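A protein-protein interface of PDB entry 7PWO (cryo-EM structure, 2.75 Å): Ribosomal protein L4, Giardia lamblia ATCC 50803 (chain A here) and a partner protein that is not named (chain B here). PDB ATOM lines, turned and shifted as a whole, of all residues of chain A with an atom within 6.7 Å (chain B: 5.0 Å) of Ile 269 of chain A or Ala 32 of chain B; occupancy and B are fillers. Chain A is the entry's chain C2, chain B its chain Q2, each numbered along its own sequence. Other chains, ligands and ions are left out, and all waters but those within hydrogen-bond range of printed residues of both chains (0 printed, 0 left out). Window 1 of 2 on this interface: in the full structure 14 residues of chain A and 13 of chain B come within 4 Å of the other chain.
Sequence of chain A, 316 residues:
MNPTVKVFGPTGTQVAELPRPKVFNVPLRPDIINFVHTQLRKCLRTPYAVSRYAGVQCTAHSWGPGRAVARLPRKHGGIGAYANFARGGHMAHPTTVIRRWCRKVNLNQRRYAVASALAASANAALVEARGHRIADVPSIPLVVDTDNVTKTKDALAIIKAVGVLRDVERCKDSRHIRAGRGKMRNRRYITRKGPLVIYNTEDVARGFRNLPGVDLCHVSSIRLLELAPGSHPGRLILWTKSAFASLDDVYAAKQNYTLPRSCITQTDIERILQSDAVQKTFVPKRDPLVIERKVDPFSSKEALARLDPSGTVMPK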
ATOM      1  N   ILE A 264     -10.829   9.050  -0.023  1.00  0.00           N
ATOM      2  CA  ILE A 264      -9.741   9.724   0.681  1.00  0.00           C
ATOM      3  C   ILE A 264      -8.365   9.345   0.161  1.00  0.00           C
ATOM      4  O   ILE A 264      -8.222   8.454  -0.683  1.00  0.00           O
ATOM      5  CB  ILE A 264      -9.807   9.429   2.181  1.00  0.00           C
ATOM      6  CG1 ILE A 264      -9.600   7.927   2.368  1.00  0.00           C
ATOM      7  CG2 ILE A 264     -11.073   9.995   2.800  1.00  0.00           C
ATOM      8  CD1 ILE A 264      -9.509   7.527   3.733  1.00  0.00           C
ATOM      9  N   THR A 265      -7.350  10.034   0.672  1.00  0.00           N
ATOM     10  CA  THR A 265      -5.957   9.850   0.303  1.00  0.00           C
ATOM     11  C   THR A 265      -5.121   9.519   1.543  1.00  0.00           C
ATOM     12  O   THR A 265      -5.568   9.623   2.694  1.00  0.00           O
ATOM     13  CB  THR A 265      -5.436  11.115  -0.399  1.00  0.00           C
ATOM     14  OG1 THR A 265      -6.392  11.537  -1.377  1.00  0.00           O
ATOM     15  CG2 THR A 265      -4.131  10.865  -1.122  1.00  0.00           C
ATOM     16  N   GLN A 266      -3.881   9.103   1.286  1.00  0.00           N
ATOM     17  CA  GLN A 266      -2.920   8.818   2.343  1.00  0.00           C
ATOM     18  C   GLN A 266      -2.638  10.043   3.203  1.00  0.00           C
ATOM     19  O   GLN A 266      -2.320   9.896   4.389  1.00  0.00           O
ATOM     20  CB  GLN A 266      -1.670   8.232   1.679  1.00  0.00           C
ATOM     21  CG  GLN A 266      -0.656   7.535   2.551  1.00  0.00           C
ATOM     22  CD  GLN A 266       0.542   8.396   2.798  1.00  0.00           C
ATOM     23  OE1 GLN A 266       0.803   9.324   2.036  1.00  0.00           O
ATOM     24  NE2 GLN A 266       1.302   8.086   3.840  1.00  0.00           N
ATOM     25  N   THR A 267      -2.825  11.246   2.658  1.00  0.00           N
ATOM     26  CA  THR A 267      -2.820  12.442   3.496  1.00  0.00           C
ATOM     27  C   THR A 267      -3.938  12.393   4.530  1.00  0.00           C
ATOM     28  O   THR A 267      -3.737  12.746   5.699  1.00  0.00           O
ATOM     29  CB  THR A 267      -2.959  13.687   2.623  1.00  0.00           C
ATOM     30  OG1 THR A 267      -1.996  13.632   1.561  1.00  0.00           O
ATOM     31  CG2 THR A 267      -2.734  14.942   3.454  1.00  0.00           C
ATOM     32  N   ASP A 268      -5.121  11.939   4.119  1.00  0.00           N
ATOM     33  CA  ASP A 268      -6.253  11.868   5.032  1.00  0.00           C
ATOM     34  C   ASP A 268      -6.064  10.780   6.086  1.00  0.00           C
ATOM     35  O   ASP A 268      -6.415  10.982   7.257  1.00  0.00           O
ATOM     36  CB  ASP A 268      -7.537  11.664   4.229  1.00  0.00           C
ATOM     37  CG  ASP A 268      -7.707  12.710   3.132  1.00  0.00           C
ATOM     38  OD1 ASP A 268      -6.902  13.664   3.081  1.00  0.00           O
ATOM     39  OD2 ASP A 268      -8.654  12.592   2.330  1.00  0.00           O
ATOM     40  N   ILE A 269      -5.496   9.631   5.701  1.00  0.00           N
ATOM     41  CA  ILE A 269      -5.165   8.605   6.696  1.00  0.00           C
ATOM     42  C   ILE A 269      -4.154   9.138   7.704  1.00  0.00           C
ATOM     43  O   ILE A 269      -4.281   8.919   8.921  1.00  0.00           O
ATOM     44  CB  ILE A 269      -4.639   7.321   6.028  1.00  0.00           C
ATOM     45  CG1 ILE A 269      -5.536   6.859   4.884  1.00  0.00           C
ATOM     46  CG2 ILE A 269      -4.553   6.219   7.046  1.00  0.00           C
ATOM     47  CD1 ILE A 269      -6.858   6.410   5.382  1.00  0.00           C
ATOM     48  N   GLU A 270      -3.122   9.827   7.211  1.00  0.00           N
ATOM     49  CA  GLU A 270      -2.106  10.386   8.090  1.00  0.00           C
ATOM     50  C   GLU A 270      -2.725  11.353   9.094  1.00  0.00           C
ATOM     51  O   GLU A 270      -2.439  11.294  10.305  1.00  0.00           O
ATOM     52  CB  GLU A 270      -1.049  11.061   7.223  1.00  0.00           C
ATOM     53  CG  GLU A 270      -0.044  11.916   7.935  1.00  0.00           C
ATOM     54  CD  GLU A 270       0.624  12.887   6.985  1.00  0.00           C
ATOM     55  OE1 GLU A 270      -0.107  13.529   6.201  1.00  0.00           O
ATOM     56  OE2 GLU A 270       1.863  13.027   7.032  1.00  0.00           O
ATOM     57  N   ARG A 271      -3.601  12.239   8.608  1.00  0.00           N
ATOM     58  CA  ARG A 271      -4.253  13.196   9.495  1.00  0.00           C
ATOM     59  C   ARG A 271      -5.098  12.496  10.546  1.00  0.00           C
ATOM     60  O   ARG A 271      -5.042  12.849  11.731  1.00  0.00           O
ATOM     61  CB  ARG A 271      -5.113  14.172   8.699  1.00  0.00           C
ATOM     62  CG  ARG A 271      -5.836  15.167   9.591  1.00  0.00           C
ATOM     63  CD  ARG A 271      -6.918  15.923   8.851  1.00  0.00           C
ATOM     64  NE  ARG A 271      -8.244  15.378   9.122  1.00  0.00           N
ATOM     65  CZ  ARG A 271      -8.888  14.550   8.304  1.00  0.00           C
ATOM     66  NH1 ARG A 271     -10.091  14.098   8.627  1.00  0.00           N
ATOM     67  NH2 ARG A 271      -8.335  14.184   7.158  1.00  0.00           N
ATOM     68  N   ILE A 272      -5.892  11.503  10.135  1.00  0.00           N
ATOM     69  CA  ILE A 272      -6.728  10.808  11.107  1.00  0.00           C
ATOM     70  C   ILE A 272      -5.858  10.218  12.205  1.00  0.00           C
ATOM     71  O   ILE A 272      -6.085  10.455  13.397  1.00  0.00           O
ATOM     72  CB  ILE A 272      -7.572   9.713  10.435  1.00  0.00           C
ATOM     73  CG1 ILE A 272      -8.550  10.283   9.416  1.00  0.00           C
ATOM     74  CG2 ILE A 272      -8.382   9.013  11.479  1.00  0.00           C
ATOM     75  CD1 ILE A 272      -9.191   9.211   8.576  1.00  0.00           C
ATOM     76  N   LEU A 273      -4.817   9.481  11.812  1.00  0.00           N
ATOM     77  CA  LEU A 273      -4.015   8.753  12.790  1.00  0.00           C
ATOM     78  C   LEU A 273      -3.361   9.692  13.794  1.00  0.00           C
ATOM     79  O   LEU A 273      -3.350   9.412  14.998  1.00  0.00           O
ATOM     80  CB  LEU A 273      -2.952   7.924  12.079  1.00  0.00           C
ATOM     81  CG  LEU A 273      -3.392   6.530  11.653  1.00  0.00           C
ATOM     82  CD1 LEU A 273      -2.225   5.815  11.014  1.00  0.00           C
ATOM     83  CD2 LEU A 273      -3.926   5.768  12.850  1.00  0.00           C
ATOM     84  N   GLN A 274      -2.802  10.809  13.327  1.00  0.00           N
ATOM     85  CA  GLN A 274      -2.206  11.737  14.283  1.00  0.00           C
ATOM     86  C   GLN A 274      -3.222  12.600  15.030  1.00  0.00           C
ATOM     87  O   GLN A 274      -2.848  13.237  16.018  1.00  0.00           O
ATOM     88  CB  GLN A 274      -1.139  12.585  13.588  1.00  0.00           C
ATOM     89  CG  GLN A 274       0.159  11.817  13.291  1.00  0.00           C
ATOM     90  CD  GLN A 274       0.052  10.727  12.243  1.00  0.00           C
ATOM     91  OE1 GLN A 274       0.311   9.564  12.545  1.00  0.00           O
ATOM     92  NE2 GLN A 274      -0.334  11.084  11.022  1.00  0.00           N
ATOM     93  N   LEU B  28      -4.127   1.333   1.774  1.00  0.00           N
ATOM     94  CA  LEU B  28      -4.101   2.349   2.829  1.00  0.00           C
ATOM     95  C   LEU B  28      -4.902   1.943   4.063  1.00  0.00           C
ATOM     96  O   LEU B  28      -4.428   2.105   5.198  1.00  0.00           O
ATOM     97  CB  LEU B  28      -4.569   3.692   2.266  1.00  0.00           C
ATOM     98  CG  LEU B  28      -3.563   4.513   1.453  1.00  0.00           C
ATOM     99  CD1 LEU B  28      -3.176   4.006   0.101  1.00  0.00           C
ATOM    100  CD2 LEU B  28      -4.245   5.830   1.244  1.00  0.00           C
ATOM    101  N   LEU B  29      -6.117   1.421   3.876  1.00  0.00           N
ATOM    102  CA  LEU B  29      -6.880   0.964   5.037  1.00  0.00           C
ATOM    103  C   LEU B  29      -6.151  -0.151   5.779  1.00  0.00           C
ATOM    104  O   LEU B  29      -6.158  -0.194   7.020  1.00  0.00           O
ATOM    105  CB  LEU B  29      -8.269   0.491   4.610  1.00  0.00           C
ATOM    106  CG  LEU B  29      -9.246   1.507   4.054  1.00  0.00           C
ATOM    107  CD1 LEU B  29     -10.459   0.767   3.585  1.00  0.00           C
ATOM    108  CD2 LEU B  29      -9.619   2.466   5.153  1.00  0.00           C
ATOM    109  N   HIS B  30      -5.504  -1.056   5.040  1.00  0.00           N
ATOM    110  CA  HIS B  30      -4.735  -2.117   5.681  1.00  0.00           C
ATOM    111  C   HIS B  30      -3.569  -1.581   6.503  1.00  0.00           C
ATOM    112  O   HIS B  30      -3.407  -1.967   7.665  1.00  0.00           O
ATOM    113  CB  HIS B  30      -4.248  -3.121   4.643  1.00  0.00           C
ATOM    114  CG  HIS B  30      -3.562  -4.300   5.245  1.00  0.00           C
ATOM    115  ND1 HIS B  30      -2.212  -4.307   5.522  1.00  0.00           N
ATOM    116  CD2 HIS B  30      -4.052  -5.450   5.754  1.00  0.00           C
ATOM    117  CE1 HIS B  30      -1.888  -5.447   6.099  1.00  0.00           C
ATOM    118  NE2 HIS B  30      -2.988  -6.159   6.252  1.00  0.00           N
ATOM    119  N   ASN B  31      -2.728  -0.721   5.923  1.00  0.00           N
ATOM    120  CA  ASN B  31      -1.618  -0.193   6.715  1.00  0.00           C
ATOM    121  C   ASN B  31      -2.123   0.531   7.958  1.00  0.00           C
ATOM    122  O   ASN B  31      -1.559   0.366   9.051  1.00  0.00           O
ATOM    123  CB  ASN B  31      -0.708   0.729   5.896  1.00  0.00           C
ATOM    124  CG  ASN B  31       0.000   0.010   4.766  1.00  0.00           C
ATOM    125  OD1 ASN B  31      -0.225   0.282   3.590  1.00  0.00           O
ATOM    126  ND2 ASN B  31       0.868  -0.924   5.127  1.00  0.00           N
ATOM    127  N   ALA B  32      -3.202   1.308   7.823  1.00  0.00           N
ATOM    128  CA  ALA B  32      -3.698   2.072   8.965  1.00  0.00           C
ATOM    129  C   ALA B  32      -4.180   1.161  10.085  1.00  0.00           C
ATOM    130  O   ALA B  32      -3.807   1.334  11.252  1.00  0.00           O
ATOM    131  CB  ALA B  32      -4.810   3.012   8.515  1.00  0.00           C
ATOM    132  N   PHE B  33      -5.000   0.175   9.755  1.00  0.00           N
ATOM    133  CA  PHE B  33      -5.527  -0.680  10.809  1.00  0.00           C
ATOM    134  C   PHE B  33      -4.448  -1.584  11.394  1.00  0.00           C
ATOM    135  O   PHE B  33      -4.504  -1.922  12.582  1.00  0.00           O
ATOM    136  CB  PHE B  33      -6.702  -1.475  10.269  1.00  0.00           C
ATOM    137  CG  PHE B  33      -8.012  -0.773  10.428  1.00  0.00           C
ATOM    138  CD1 PHE B  33      -8.525  -0.515  11.679  1.00  0.00           C
ATOM    139  CD2 PHE B  33      -8.718  -0.334   9.324  1.00  0.00           C
ATOM    140  CE1 PHE B  33      -9.728   0.149  11.822  1.00  0.00           C
ATOM    141  CE2 PHE B  33      -9.923   0.321   9.474  1.00  0.00           C
ATOM    142  CZ  PHE B  33     -10.425   0.551  10.717  1.00  0.00           C
ATOM    143  N   LYS B  34      -3.433  -1.937  10.601  1.00  0.00           N
ATOM    144  CA  LYS B  34      -2.296  -2.677  11.136  1.00  0.00           C
ATOM    145  C   LYS B  34      -1.537  -1.848  12.170  1.00  0.00           C
ATOM    146  O   LYS B  34      -1.111  -2.373  13.209  1.00  0.00           O
ATOM    147  CB  LYS B  34      -1.381  -3.093   9.988  1.00  0.00           C
ATOM    148  CG  LYS B  34      -0.529  -4.298  10.263  1.00  0.00           C
ATOM    149  CD  LYS B  34       0.513  -4.482   9.187  1.00  0.00           C
ATOM    150  CE  LYS B  34       1.704  -5.231   9.722  1.00  0.00           C
ATOM    151  NZ  LYS B  34       2.169  -4.695  11.030  1.00  0.00           N
ATOM    152  N   VAL B  35      -1.378  -0.545  11.915  1.00  0.00           N
ATOM    153  CA  VAL B  35      -0.767   0.345  12.908  1.00  0.00           C
ATOM    154  C   VAL B  35      -1.602   0.395  14.184  1.00  0.00           C
ATOM    155  O   VAL B  35      -1.072   0.328  15.303  1.00  0.00           O
ATOM    156  CB  VAL B  35      -0.568   1.755  12.324  1.00  0.00           C
ATOM    157  CG1 VAL B  35      -0.050   2.686  13.385  1.00  0.00           C
ATOM    158  CG2 VAL B  35       0.408   1.716  11.173  1.00  0.00           C
ATOM    159  N   VAL B  36      -2.918   0.556  14.038  1.00  0.00           N
ATOM    160  CA  VAL B  36      -3.772   0.627  15.223  1.00  0.00           C
ATOM    161  C   VAL B  36      -3.654  -0.646  16.051  1.00  0.00           C
ATOM    162  O   VAL B  36      -3.538  -0.587  17.282  1.00  0.00           O
ATOM    163  CB  VAL B  36      -5.232   0.924  14.836  1.00  0.00           C
ATOM    164  CG1 VAL B  36      -6.113   0.877  16.056  1.00  0.00           C
ATOM    165  CG2 VAL B  36      -5.333   2.308  14.231  1.00  0.00           C
ATOM    166  N   ASP B 123     -12.776   4.344   6.622  1.00  0.00           N
ATOM    167  CA  ASP B 123     -12.090   5.516   7.155  1.00  0.00           C
ATOM    168  C   ASP B 123     -12.974   6.264   8.146  1.00  0.00           C
ATOM    169  O   ASP B 123     -12.487   6.791   9.152  1.00  0.00           O
ATOM    170  CB  ASP B 123     -11.645   6.436   6.025  1.00  0.00           C
ATOM    171  CG  ASP B 123     -12.796   6.943   5.178  1.00  0.00           C
ATOM    172  OD1 ASP B 123     -13.947   6.545   5.415  1.00  0.00           O
ATOM    173  OD2 ASP B 123     -12.551   7.742   4.260  1.00  0.00           O
ATOM    174  N   LEU B 126     -12.556   4.199  11.184  1.00  0.00           N
ATOM    175  CA  LEU B 126     -11.256   4.382  11.807  1.00  0.00           C
ATOM    176  C   LEU B 126     -11.098   5.756  12.438  1.00  0.00           C
ATOM    177  O   LEU B 126     -10.274   5.910  13.343  1.00  0.00           O
ATOM    178  CB  LEU B 126     -10.162   4.091  10.774  1.00  0.00           C
ATOM    179  CG  LEU B 126      -8.684   4.038  11.145  1.00  0.00           C
ATOM    180  CD1 LEU B 126      -7.945   3.131  10.206  1.00  0.00           C
ATOM    181  CD2 LEU B 126      -8.112   5.435  10.959  1.00  0.00           C
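The backbone NH of Thr 265 of chain A lies within hydrogen-bond range of the side-chain carboxylate of Asp 268 of chain A (3.3 Å).
Among the printed residues, pairs that only touch across the chains: Ile 264 of chain A with Asp 123 of chain B (3.1 Å), Thr 265 of chain A with Leu 28 of chain B (3.8 Å), Gln 266 of chain A with Leu 28 of chain B (3.3 Å), Ile 269 of chain A with Leu 28 of chain B (3.997 Å), Ile 269 of chain A with Ala 32 of chain B (3.5 Å), Ile 272 of chain A with Leu 126 of chain B (3.6 Å) and Leu 273 of chain A with Val 36 of chain B (3.98 Å).
Printed residues of chain B within 4 Å of Ile 269 of chain A: Leu 28 and Ala 32.
Of chain A, only Ile 269 (3.5 Å) comes within 4 Å of Ala 32 of chain B.
Of the printed residues of chain B, Thr 265 of chain A touches Leu 28 (3.8 Å).
Printed residues of chain B within 4 Å of Ile 272 of chain A: Leu 126 (3.6 Å).
Printed residues of chain B within 4 Å of Gln 266 of chain A: Leu 28.
Of the printed residues of chain A, Leu 28 of chain B touches Thr 265 (3.8 Å), Gln 266 (3.3 Å) and Ile 269 (3.997 Å).
Of the printed residues of chain A, Val 36 of chain B touches Leu 273.
Leu 29 of chain B touches none of the printed residues of chain A.
Arg 271 of chain A touches none of the printed residues of chain B.
The nearest printed residue of chain B that does not touch Ile 269 of chain A is Leu 29 of chain B (4.8 Å).
The nearest residue of chain A that does not touch Ala 32 of chain B is Leu 273 of chain A (4.5 Å).
The nearest printed residue of chain A that does not touch Asp 123 of chain B is Ile 272 of chain A (4.1 Å).
Of the 11 printed residues of chain A, 6 touch a printed residue of chain B.
Hydrophobic or aromatic side chains of chain A within 4 Å of the printed part of chain B: Ile 264, Ile 269, Ile 272 and Leu 273.
Hydrophobic or aromatic side chains of chain B within 4 Å of the printed part of chain A: Leu 28, Ala 32, Val 36 and Leu 126.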
